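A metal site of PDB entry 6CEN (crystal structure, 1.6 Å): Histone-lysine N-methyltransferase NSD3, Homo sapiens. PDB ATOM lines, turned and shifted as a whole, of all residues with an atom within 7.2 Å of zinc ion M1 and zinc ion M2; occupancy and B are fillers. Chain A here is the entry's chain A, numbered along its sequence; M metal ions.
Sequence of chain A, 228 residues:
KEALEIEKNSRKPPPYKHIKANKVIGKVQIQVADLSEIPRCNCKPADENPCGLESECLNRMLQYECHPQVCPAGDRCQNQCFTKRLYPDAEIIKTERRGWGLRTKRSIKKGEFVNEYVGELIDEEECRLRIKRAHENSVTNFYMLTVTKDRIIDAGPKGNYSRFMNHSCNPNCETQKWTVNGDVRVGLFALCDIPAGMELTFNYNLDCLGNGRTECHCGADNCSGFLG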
ATOM      1  N   ARG A  40      27.037   6.556  23.861  1.00  0.00           N
ATOM      2  CA  ARG A  40      26.830   7.916  24.306  1.00  0.00           C
ATOM      3  C   ARG A  40      28.175   8.567  24.565  1.00  0.00           C
ATOM      4  O   ARG A  40      28.996   8.021  25.274  1.00  0.00           O
ATOM      5  CB  ARG A  40      26.016   7.914  25.591  1.00  0.00           C
ATOM      6  CG  ARG A  40      25.632   9.292  26.091  1.00  0.00           C
ATOM      7  CD  ARG A  40      25.163   9.272  27.545  1.00  0.00           C
ATOM      8  NE  ARG A  40      23.832   8.673  27.652  1.00  0.00           N
ATOM      9  CZ  ARG A  40      23.558   7.393  27.900  1.00  0.00           C
ATOM     10  NH1 ARG A  40      24.525   6.475  28.082  1.00  0.00           N
ATOM     11  NH2 ARG A  40      22.285   6.998  27.969  1.00  0.00           N
ATOM     12  N   CYS A  41      28.399   9.744  23.974  1.00  0.00           N
ATOM     13  CA  CYS A  41      29.608  10.506  24.211  1.00  0.00           C
ATOM     14  C   CYS A  41      29.491  11.331  25.508  1.00  0.00           C
ATOM     15  O   CYS A  41      28.426  11.361  26.139  1.00  0.00           O
ATOM     16  CB  CYS A  41      29.883  11.414  23.026  1.00  0.00           C
ATOM     17  SG  CYS A  41      28.808  12.856  22.868  1.00  0.00           S
ATOM     18  N   ASN A  42      30.582  12.005  25.867  1.00  0.00           N
ATOM     19  CA  ASN A  42      30.631  12.841  27.068  1.00  0.00           C
ATOM     20  C   ASN A  42      30.608  14.353  26.795  1.00  0.00           C
ATOM     21  O   ASN A  42      30.897  15.145  27.696  1.00  0.00           O
ATOM     22  CB  ASN A  42      31.865  12.483  27.890  1.00  0.00           C
ATOM     23  CG  ASN A  42      31.761  11.114  28.537  1.00  0.00           C
ATOM     24  OD1 ASN A  42      30.674  10.661  28.898  1.00  0.00           O
ATOM     25  ND2 ASN A  42      32.892  10.458  28.692  1.00  0.00           N
ATOM     26  N   CYS A  43      30.244  14.758  25.566  1.00  0.00           N
ATOM     27  CA  CYS A  43      30.148  16.175  25.231  1.00  0.00           C
ATOM     28  C   CYS A  43      28.985  16.770  26.013  1.00  0.00           C
ATOM     29  O   CYS A  43      28.067  16.048  26.434  1.00  0.00           O
ATOM     30  CB  CYS A  43      29.936  16.410  23.724  1.00  0.00           C
ATOM     31  SG  CYS A  43      31.225  15.762  22.618  1.00  0.00           S
ATOM     32  N   LYS A  44      29.034  18.076  26.227  1.00  0.00           N
ATOM     33  CA  LYS A  44      28.004  18.801  26.992  1.00  0.00           C
ATOM     34  C   LYS A  44      27.148  19.665  26.061  1.00  0.00           C
ATOM     35  O   LYS A  44      27.671  20.290  25.151  1.00  0.00           O
ATOM     36  CB  LYS A  44      28.653  19.657  28.086  1.00  0.00           C
ATOM     37  CG  LYS A  44      28.839  18.899  29.390  1.00  0.00           C
ATOM     38  CD  LYS A  44      29.668  19.676  30.394  1.00  0.00           C
ATOM     39  CE  LYS A  44      29.499  19.105  31.790  1.00  0.00           C
ATOM     40  NZ  LYS A  44      30.511  19.634  32.757  1.00  0.00           N
ATOM     41  N   ASP A  47      28.332  23.140  25.210  1.00  0.00           N
ATOM     42  CA  ASP A  47      29.563  23.301  24.408  1.00  0.00           C
ATOM     43  C   ASP A  47      29.379  24.149  23.167  1.00  0.00           C
ATOM     44  O   ASP A  47      28.301  24.167  22.583  1.00  0.00           O
ATOM     45  CB  ASP A  47      30.107  21.933  23.938  1.00  0.00           C
ATOM     46  CG  ASP A  47      30.702  21.102  25.071  1.00  0.00           C
ATOM     47  OD1 ASP A  47      30.911  21.628  26.183  1.00  0.00           O
ATOM     48  OD2 ASP A  47      30.967  19.897  24.835  1.00  0.00           O
ATOM     49  N   PRO A  50      29.128  21.223  19.791  1.00  0.00           N
ATOM     50  CA  PRO A  50      29.133  19.931  20.463  1.00  0.00           C
ATOM     51  C   PRO A  50      29.243  18.804  19.434  1.00  0.00           C
ATOM     52  O   PRO A  50      28.536  18.817  18.433  1.00  0.00           O
ATOM     53  CB  PRO A  50      27.791  19.893  21.201  1.00  0.00           C
ATOM     54  CG  PRO A  50      26.940  20.908  20.528  1.00  0.00           C
ATOM     55  CD  PRO A  50      27.839  21.919  19.918  1.00  0.00           C
ATOM     56  N   CYS A  51      30.151  17.873  19.709  1.00  0.00           N
ATOM     57  CA  CYS A  51      30.440  16.749  18.828  1.00  0.00           C
ATOM     58  C   CYS A  51      30.988  17.154  17.451  1.00  0.00           C
ATOM     59  O   CYS A  51      30.897  16.375  16.498  1.00  0.00           O
ATOM     60  CB  CYS A  51      29.214  15.855  18.669  1.00  0.00           C
ATOM     61  SG  CYS A  51      28.462  15.426  20.259  1.00  0.00           S
ATOM     62  N   GLY A  52      31.589  18.336  17.369  1.00  0.00           N
ATOM     63  CA  GLY A  52      32.101  18.860  16.093  1.00  0.00           C
ATOM     64  C   GLY A  52      33.497  18.361  15.757  1.00  0.00           C
ATOM     65  O   GLY A  52      34.119  17.651  16.535  1.00  0.00           O
ATOM     66  N   SER A  55      36.115  18.948  18.319  1.00  0.00           N
ATOM     67  CA  SER A  55      35.745  18.544  19.677  1.00  0.00           C
ATOM     68  C   SER A  55      36.544  17.355  20.132  1.00  0.00           C
ATOM     69  O   SER A  55      37.247  16.699  19.354  1.00  0.00           O
ATOM     70  CB  SER A  55      34.242  18.214  19.746  1.00  0.00           C
ATOM     71  OG  SER A  55      33.935  17.010  19.066  1.00  0.00           O
ATOM     72  N   GLU A  56      36.412  17.057  21.421  1.00  0.00           N
ATOM     73  CA  GLU A  56      36.993  15.853  21.998  1.00  0.00           C
ATOM     74  C   GLU A  56      36.116  14.602  21.773  1.00  0.00           C
ATOM     75  O   GLU A  56      36.417  13.551  22.346  1.00  0.00           O
ATOM     76  CB  GLU A  56      37.249  16.072  23.517  1.00  0.00           C
ATOM     77  CG  GLU A  56      36.040  15.963  24.466  1.00  0.00           C
ATOM     78  CD  GLU A  56      35.017  17.088  24.352  1.00  0.00           C
ATOM     79  OE1 GLU A  56      35.275  18.086  23.632  1.00  0.00           O
ATOM     80  OE2 GLU A  56      33.942  16.987  24.994  1.00  0.00           O
ATOM     81  N   CYS A  57      35.066  14.702  20.950  1.00  0.00           N
ATOM     82  CA  CYS A  57      33.936  13.776  21.016  1.00  0.00           C
ATOM     83  C   CYS A  57      34.361  12.330  20.929  1.00  0.00           C
ATOM     84  O   CYS A  57      34.999  11.941  19.944  1.00  0.00           O
ATOM     85  CB  CYS A  57      32.948  14.040  19.872  1.00  0.00           C
ATOM     86  SG  CYS A  57      31.493  13.001  19.977  1.00  0.00           S
ATOM     87  N   LEU A  58      34.027  11.548  21.952  1.00  0.00           N
ATOM     88  CA  LEU A  58      34.409  10.120  22.005  1.00  0.00           C
ATOM     89  C   LEU A  58      33.799   9.327  20.843  1.00  0.00           C
ATOM     90  O   LEU A  58      34.438   8.416  20.322  1.00  0.00           O
ATOM     91  CB  LEU A  58      33.995   9.473  23.327  1.00  0.00           C
ATOM     92  CG  LEU A  58      34.809   9.788  24.574  1.00  0.00           C
ATOM     93  CD1 LEU A  58      34.139   9.154  25.793  1.00  0.00           C
ATOM     94  CD2 LEU A  58      36.239   9.302  24.426  1.00  0.00           C
ATOM     95  N   ASN A  59      32.567   9.645  20.470  1.00  0.00           N
ATOM     96  CA  ASN A  59      31.916   8.970  19.323  1.00  0.00           C
ATOM     97  C   ASN A  59      32.643   9.297  18.009  1.00  0.00           C
ATOM     98  O   ASN A  59      33.069   8.392  17.282  1.00  0.00           O
ATOM     99  CB  ASN A  59      30.419   9.331  19.234  1.00  0.00           C
ATOM    100  CG  ASN A  59      29.557   8.524  20.195  1.00  0.00           C
ATOM    101  OD1 ASN A  59      30.039   7.644  20.913  1.00  0.00           O
ATOM    102  ND2 ASN A  59      28.242   8.767  20.169  1.00  0.00           N
ATOM    103  N   ARG A  60      32.878  10.565  17.747  1.00  0.00           N
ATOM    104  CA  ARG A  60      33.466  11.004  16.491  1.00  0.00           C
ATOM    105  C   ARG A  60      34.895  10.467  16.388  1.00  0.00           C
ATOM    106  O   ARG A  60      35.308  10.002  15.317  1.00  0.00           O
ATOM    107  CB  ARG A  60      33.440  12.535  16.407  1.00  0.00           C
ATOM    108  CG  ARG A  60      34.100  13.159  15.205  1.00  0.00           C
ATOM    109  CD  ARG A  60      33.976  14.674  15.259  1.00  0.00           C
ATOM    110  NE  ARG A  60      32.687  15.149  14.773  1.00  0.00           N
ATOM    111  CZ  ARG A  60      32.325  15.224  13.484  1.00  0.00           C
ATOM    112  NH1 ARG A  60      33.135  14.806  12.511  1.00  0.00           N
ATOM    113  NH2 ARG A  60      31.126  15.695  13.173  1.00  0.00           N
ATOM    114  N   GLU A  65      28.628   7.644  14.677  1.00  0.00           N
ATOM    115  CA  GLU A  65      27.681   8.754  14.575  1.00  0.00           C
ATOM    116  C   GLU A  65      26.812   8.778  15.815  1.00  0.00           C
ATOM    117  O   GLU A  65      26.353   7.746  16.276  1.00  0.00           O
ATOM    118  CB  GLU A  65      26.821   8.555  13.315  1.00  0.00           C
ATOM    119  CG  GLU A  65      25.634   9.519  13.234  1.00  0.00           C
ATOM    120  CD  GLU A  65      25.366  10.071  11.857  1.00  0.00           C
ATOM    121  OE1 GLU A  65      26.326  10.384  11.150  1.00  0.00           O
ATOM    122  OE2 GLU A  65      24.194  10.253  11.517  1.00  0.00           O
ATOM    123  N   CYS A  66      26.571   9.975  16.350  1.00  0.00           N
ATOM    124  CA  CYS A  66      25.620  10.134  17.461  1.00  0.00           C
ATOM    125  C   CYS A  66      24.184   9.918  17.019  1.00  0.00           C
ATOM    126  O   CYS A  66      23.834  10.194  15.876  1.00  0.00           O
ATOM    127  CB  CYS A  66      25.721  11.554  18.031  1.00  0.00           C
ATOM    128  SG  CYS A  66      27.221  11.905  18.920  1.00  0.00           S
ATOM    129  N   HIS A  67      23.357   9.433  17.945  1.00  0.00           N
ATOM    130  CA  HIS A  67      21.906   9.357  17.737  1.00  0.00           C
ATOM    131  C   HIS A  67      21.314  10.451  18.650  1.00  0.00           C
ATOM    132  O   HIS A  67      21.637  10.504  19.838  1.00  0.00           O
ATOM    133  CB  HIS A  67      21.427   7.962  18.136  1.00  0.00           C
ATOM    134  CG  HIS A  67      20.015   7.638  17.741  1.00  0.00           C
ATOM    135  ND1 HIS A  67      18.924   8.278  18.274  1.00  0.00           N
ATOM    136  CD2 HIS A  67      19.526   6.723  16.887  1.00  0.00           C
ATOM    137  CE1 HIS A  67      17.819   7.773  17.770  1.00  0.00           C
ATOM    138  NE2 HIS A  67      18.155   6.822  16.926  1.00  0.00           N
ATOM    139  N   PRO A  68      20.477  11.337  18.100  1.00  0.00           N
ATOM    140  CA  PRO A  68      20.034  12.541  18.840  1.00  0.00           C
ATOM    141  C   PRO A  68      19.260  12.251  20.150  1.00  0.00           C
ATOM    142  O   PRO A  68      19.379  13.001  21.119  1.00  0.00           O
ATOM    143  CB  PRO A  68      19.144  13.263  17.811  1.00  0.00           C
ATOM    144  CG  PRO A  68      18.703  12.220  16.876  1.00  0.00           C
ATOM    145  CD  PRO A  68      19.818  11.222  16.793  1.00  0.00           C
ATOM    146  N   VAL A  70      20.103   9.943  22.077  1.00  0.00           N
ATOM    147  CA  VAL A  70      21.119   9.420  22.981  1.00  0.00           C
ATOM    148  C   VAL A  70      22.142  10.471  23.407  1.00  0.00           C
ATOM    149  O   VAL A  70      22.575  10.491  24.556  1.00  0.00           O
ATOM    150  CB  VAL A  70      21.847   8.215  22.314  1.00  0.00           C
ATOM    151  CG1 VAL A  70      22.945   7.637  23.207  1.00  0.00           C
ATOM    152  CG2 VAL A  70      20.837   7.136  21.964  1.00  0.00           C
ATOM    153  N   CYS A  71      22.571  11.320  22.471  1.00  0.00           N
ATOM    154  CA  CYS A  71      23.694  12.227  22.718  1.00  0.00           C
ATOM    155  C   CYS A  71      23.367  13.278  23.797  1.00  0.00           C
ATOM    156  O   CYS A  71      22.302  13.849  23.752  1.00  0.00           O
ATOM    157  CB  CYS A  71      24.048  12.930  21.409  1.00  0.00           C
ATOM    158  SG  CYS A  71      25.376  14.131  21.526  1.00  0.00           S
ATOM    159  N   PRO A  72      24.285  13.551  24.753  1.00  0.00           N
ATOM    160  CA  PRO A  72      23.955  14.612  25.724  1.00  0.00           C
ATOM    161  C   PRO A  72      23.673  15.986  25.105  1.00  0.00           C
ATOM    162  O   PRO A  72      22.997  16.784  25.753  1.00  0.00           O
ATOM    163  CB  PRO A  72      25.205  14.666  26.608  1.00  0.00           C
ATOM    164  CG  PRO A  72      25.724  13.277  26.572  1.00  0.00           C
ATOM    165  CD  PRO A  72      25.509  12.841  25.141  1.00  0.00           C
ATOM    166  N   ALA A  73      24.174  16.238  23.894  1.00  0.00           N
ATOM    167  CA  ALA A  73      23.997  17.519  23.196  1.00  0.00           C
ATOM    168  C   ALA A  73      22.641  17.719  22.527  1.00  0.00           C
ATOM    169  O   ALA A  73      22.390  18.804  22.022  1.00  0.00           O
ATOM    170  CB  ALA A  73      25.106  17.721  22.152  1.00  0.00           C
ATOM    171  N   GLY A  74      21.779  16.699  22.498  1.00  0.00           N
ATOM    172  CA  GLY A  74      20.490  16.854  21.822  1.00  0.00           C
ATOM    173  C   GLY A  74      20.631  17.062  20.322  1.00  0.00           C
ATOM    174  O   GLY A  74      21.509  16.488  19.670  1.00  0.00           O
ATOM    175  N   ARG A  76      21.575  19.849  18.985  1.00  0.00           N
ATOM    176  CA  ARG A  76      22.764  20.679  18.704  1.00  0.00           C
ATOM    177  C   ARG A  76      23.967  19.846  18.221  1.00  0.00           C
ATOM    178  O   ARG A  76      24.926  20.401  17.677  1.00  0.00           O
ATOM    179  CB  ARG A  76      23.186  21.450  19.959  1.00  0.00           C
ATOM    180  CG  ARG A  76      22.206  22.528  20.402  1.00  0.00           C
ATOM    181  CD  ARG A  76      22.853  23.494  21.393  1.00  0.00           C
ATOM    182  NE  ARG A  76      23.955  24.268  20.806  1.00  0.00           N
ATOM    183  CZ  ARG A  76      25.210  24.342  21.269  1.00  0.00           C
ATOM    184  NH1 ARG A  76      25.605  23.708  22.379  1.00  0.00           N
ATOM    185  NH2 ARG A  76      26.095  25.091  20.616  1.00  0.00           N
ATOM    186  N   CYS A  77      23.918  18.531  18.456  1.00  0.00           N
ATOM    187  CA  CYS A  77      24.990  17.619  18.077  1.00  0.00           C
ATOM    188  C   CYS A  77      25.417  17.796  16.615  1.00  0.00           C
ATOM    189  O   CYS A  77      24.580  17.720  15.718  1.00  0.00           O
ATOM    190  CB  CYS A  77      24.535  16.186  18.348  1.00  0.00           C
ATOM    191  SG  CYS A  77      25.689  14.919  17.746  1.00  0.00           S
ATOM    192  N   GLN A  78      26.708  18.032  16.386  1.00  0.00           N
ATOM    193  CA  GLN A  78      27.275  18.168  15.045  1.00  0.00           C
ATOM    194  C   GLN A  78      27.856  16.853  14.472  1.00  0.00           C
ATOM    195  O   GLN A  78      28.647  16.864  13.539  1.00  0.00           O
ATOM    196  CB  GLN A  78      28.364  19.263  15.043  1.00  0.00           C
ATOM    197  CG  GLN A  78      27.850  20.572  15.624  1.00  0.00           C
ATOM    198  CD  GLN A  78      28.775  21.756  15.404  1.00  0.00           C
ATOM    199  OE1 GLN A  78      29.927  21.601  15.024  1.00  0.00           O
ATOM    200  NE2 GLN A  78      28.255  22.954  15.669  1.00  0.00           N
ATOM    201  N   ASN A  79      27.476  15.726  15.061  1.00  0.00           N
ATOM    202  CA  ASN A  79      27.911  14.402  14.607  1.00  0.00           C
ATOM    203  C   ASN A  79      26.709  13.540  14.181  1.00  0.00           C
ATOM    204  O   ASN A  79      26.560  12.398  14.632  1.00  0.00           O
ATOM    205  CB  ASN A  79      28.675  13.742  15.736  1.00  0.00           C
ATOM    206  CG  ASN A  79      29.351  12.453  15.329  1.00  0.00           C
ATOM    207  OD1 ASN A  79      29.765  12.289  14.187  1.00  0.00           O
ATOM    208  ND2 ASN A  79      29.484  11.551  16.263  1.00  0.00           N
ATOM    209  N   GLN A  80      25.872  14.105  13.310  1.00  0.00           N
ATOM    210  CA  GLN A  80      24.692  13.445  12.753  1.00  0.00           C
ATOM    211  C   GLN A  80      24.719  13.515  11.223  1.00  0.00           C
ATOM    212  O   GLN A  80      23.683  13.546  10.571  1.00  0.00           O
ATOM    213  CB  GLN A  80      23.408  14.092  13.271  1.00  0.00           C
ATOM    214  CG  GLN A  80      23.316  14.207  14.790  1.00  0.00           C
ATOM    215  CD  GLN A  80      22.022  14.874  15.209  1.00  0.00           C
ATOM    216  OE1 GLN A  80      20.950  14.321  14.995  1.00  0.00           O
ATOM    217  NE2 GLN A  80      22.110  16.103  15.727  1.00  0.00           N
HETATM  218 ZN    ZN M   1      26.683  14.045  19.638  1.00  0.00          ZN
HETATM  219 ZN    ZN M   2      30.028  14.158  21.383  1.00  0.00          ZN
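The side-chain sulfur (SG) of Cys 71 lies close to the backbone NH (N) of Ala 73, at 3.4 Å.
NE of Arg 60 is in hydrogen-bond range of O of Cys 51, 2.8 Å away.
N of Asn 79 lies close to SG of Cys 77 (3.3 Å).
The backbone carbonyl oxygen of Cys 77 lies within hydrogen-bond range of the side-chain amide nitrogen of Gln 80 (3.0 Å).
The backbone carbonyl oxygen of Asn 79 lies within hydrogen-bond range of the backbone NH of Cys 66 (3.0 Å).
The side-chain amide nitrogen (ND2) of Asn 59 lies close to the side-chain sulfur (SG) of Cys 66 (3.5 Å).
The backbone NH (N) of Cys 57 lies close to the side-chain hydroxyl (OG) of Ser 55, 3.2 Å away.
SG of Cys 57 lies close to N of Arg 60.
The nearest printed residue that does not touch zinc ion M1 is Cys 41 (4.05 Å).
Of the 29 residues printed, 4 come within 4 Å of zinc ion M2.
Zinc ion M1 is bound by the side-chain sulfur of Cys 71 (2.3 Å), the side-chain sulfur of Cys 77 (2.3 Å), the side-chain sulfur of Cys 66 (2.3 Å) and the side-chain sulfur of Cys 51 (2.3 Å).
Zinc ion M2 is bound by the side-chain sulfur of Cys 51 (2.3 Å), the side-chain sulfur of Cys 41 (2.3 Å), the side-chain sulfur of Cys 57 (2.3 Å) and the side-chain sulfur of Cys 43 (2.4 Å).
Zinc ion M2 has four donor atoms within binding distance.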
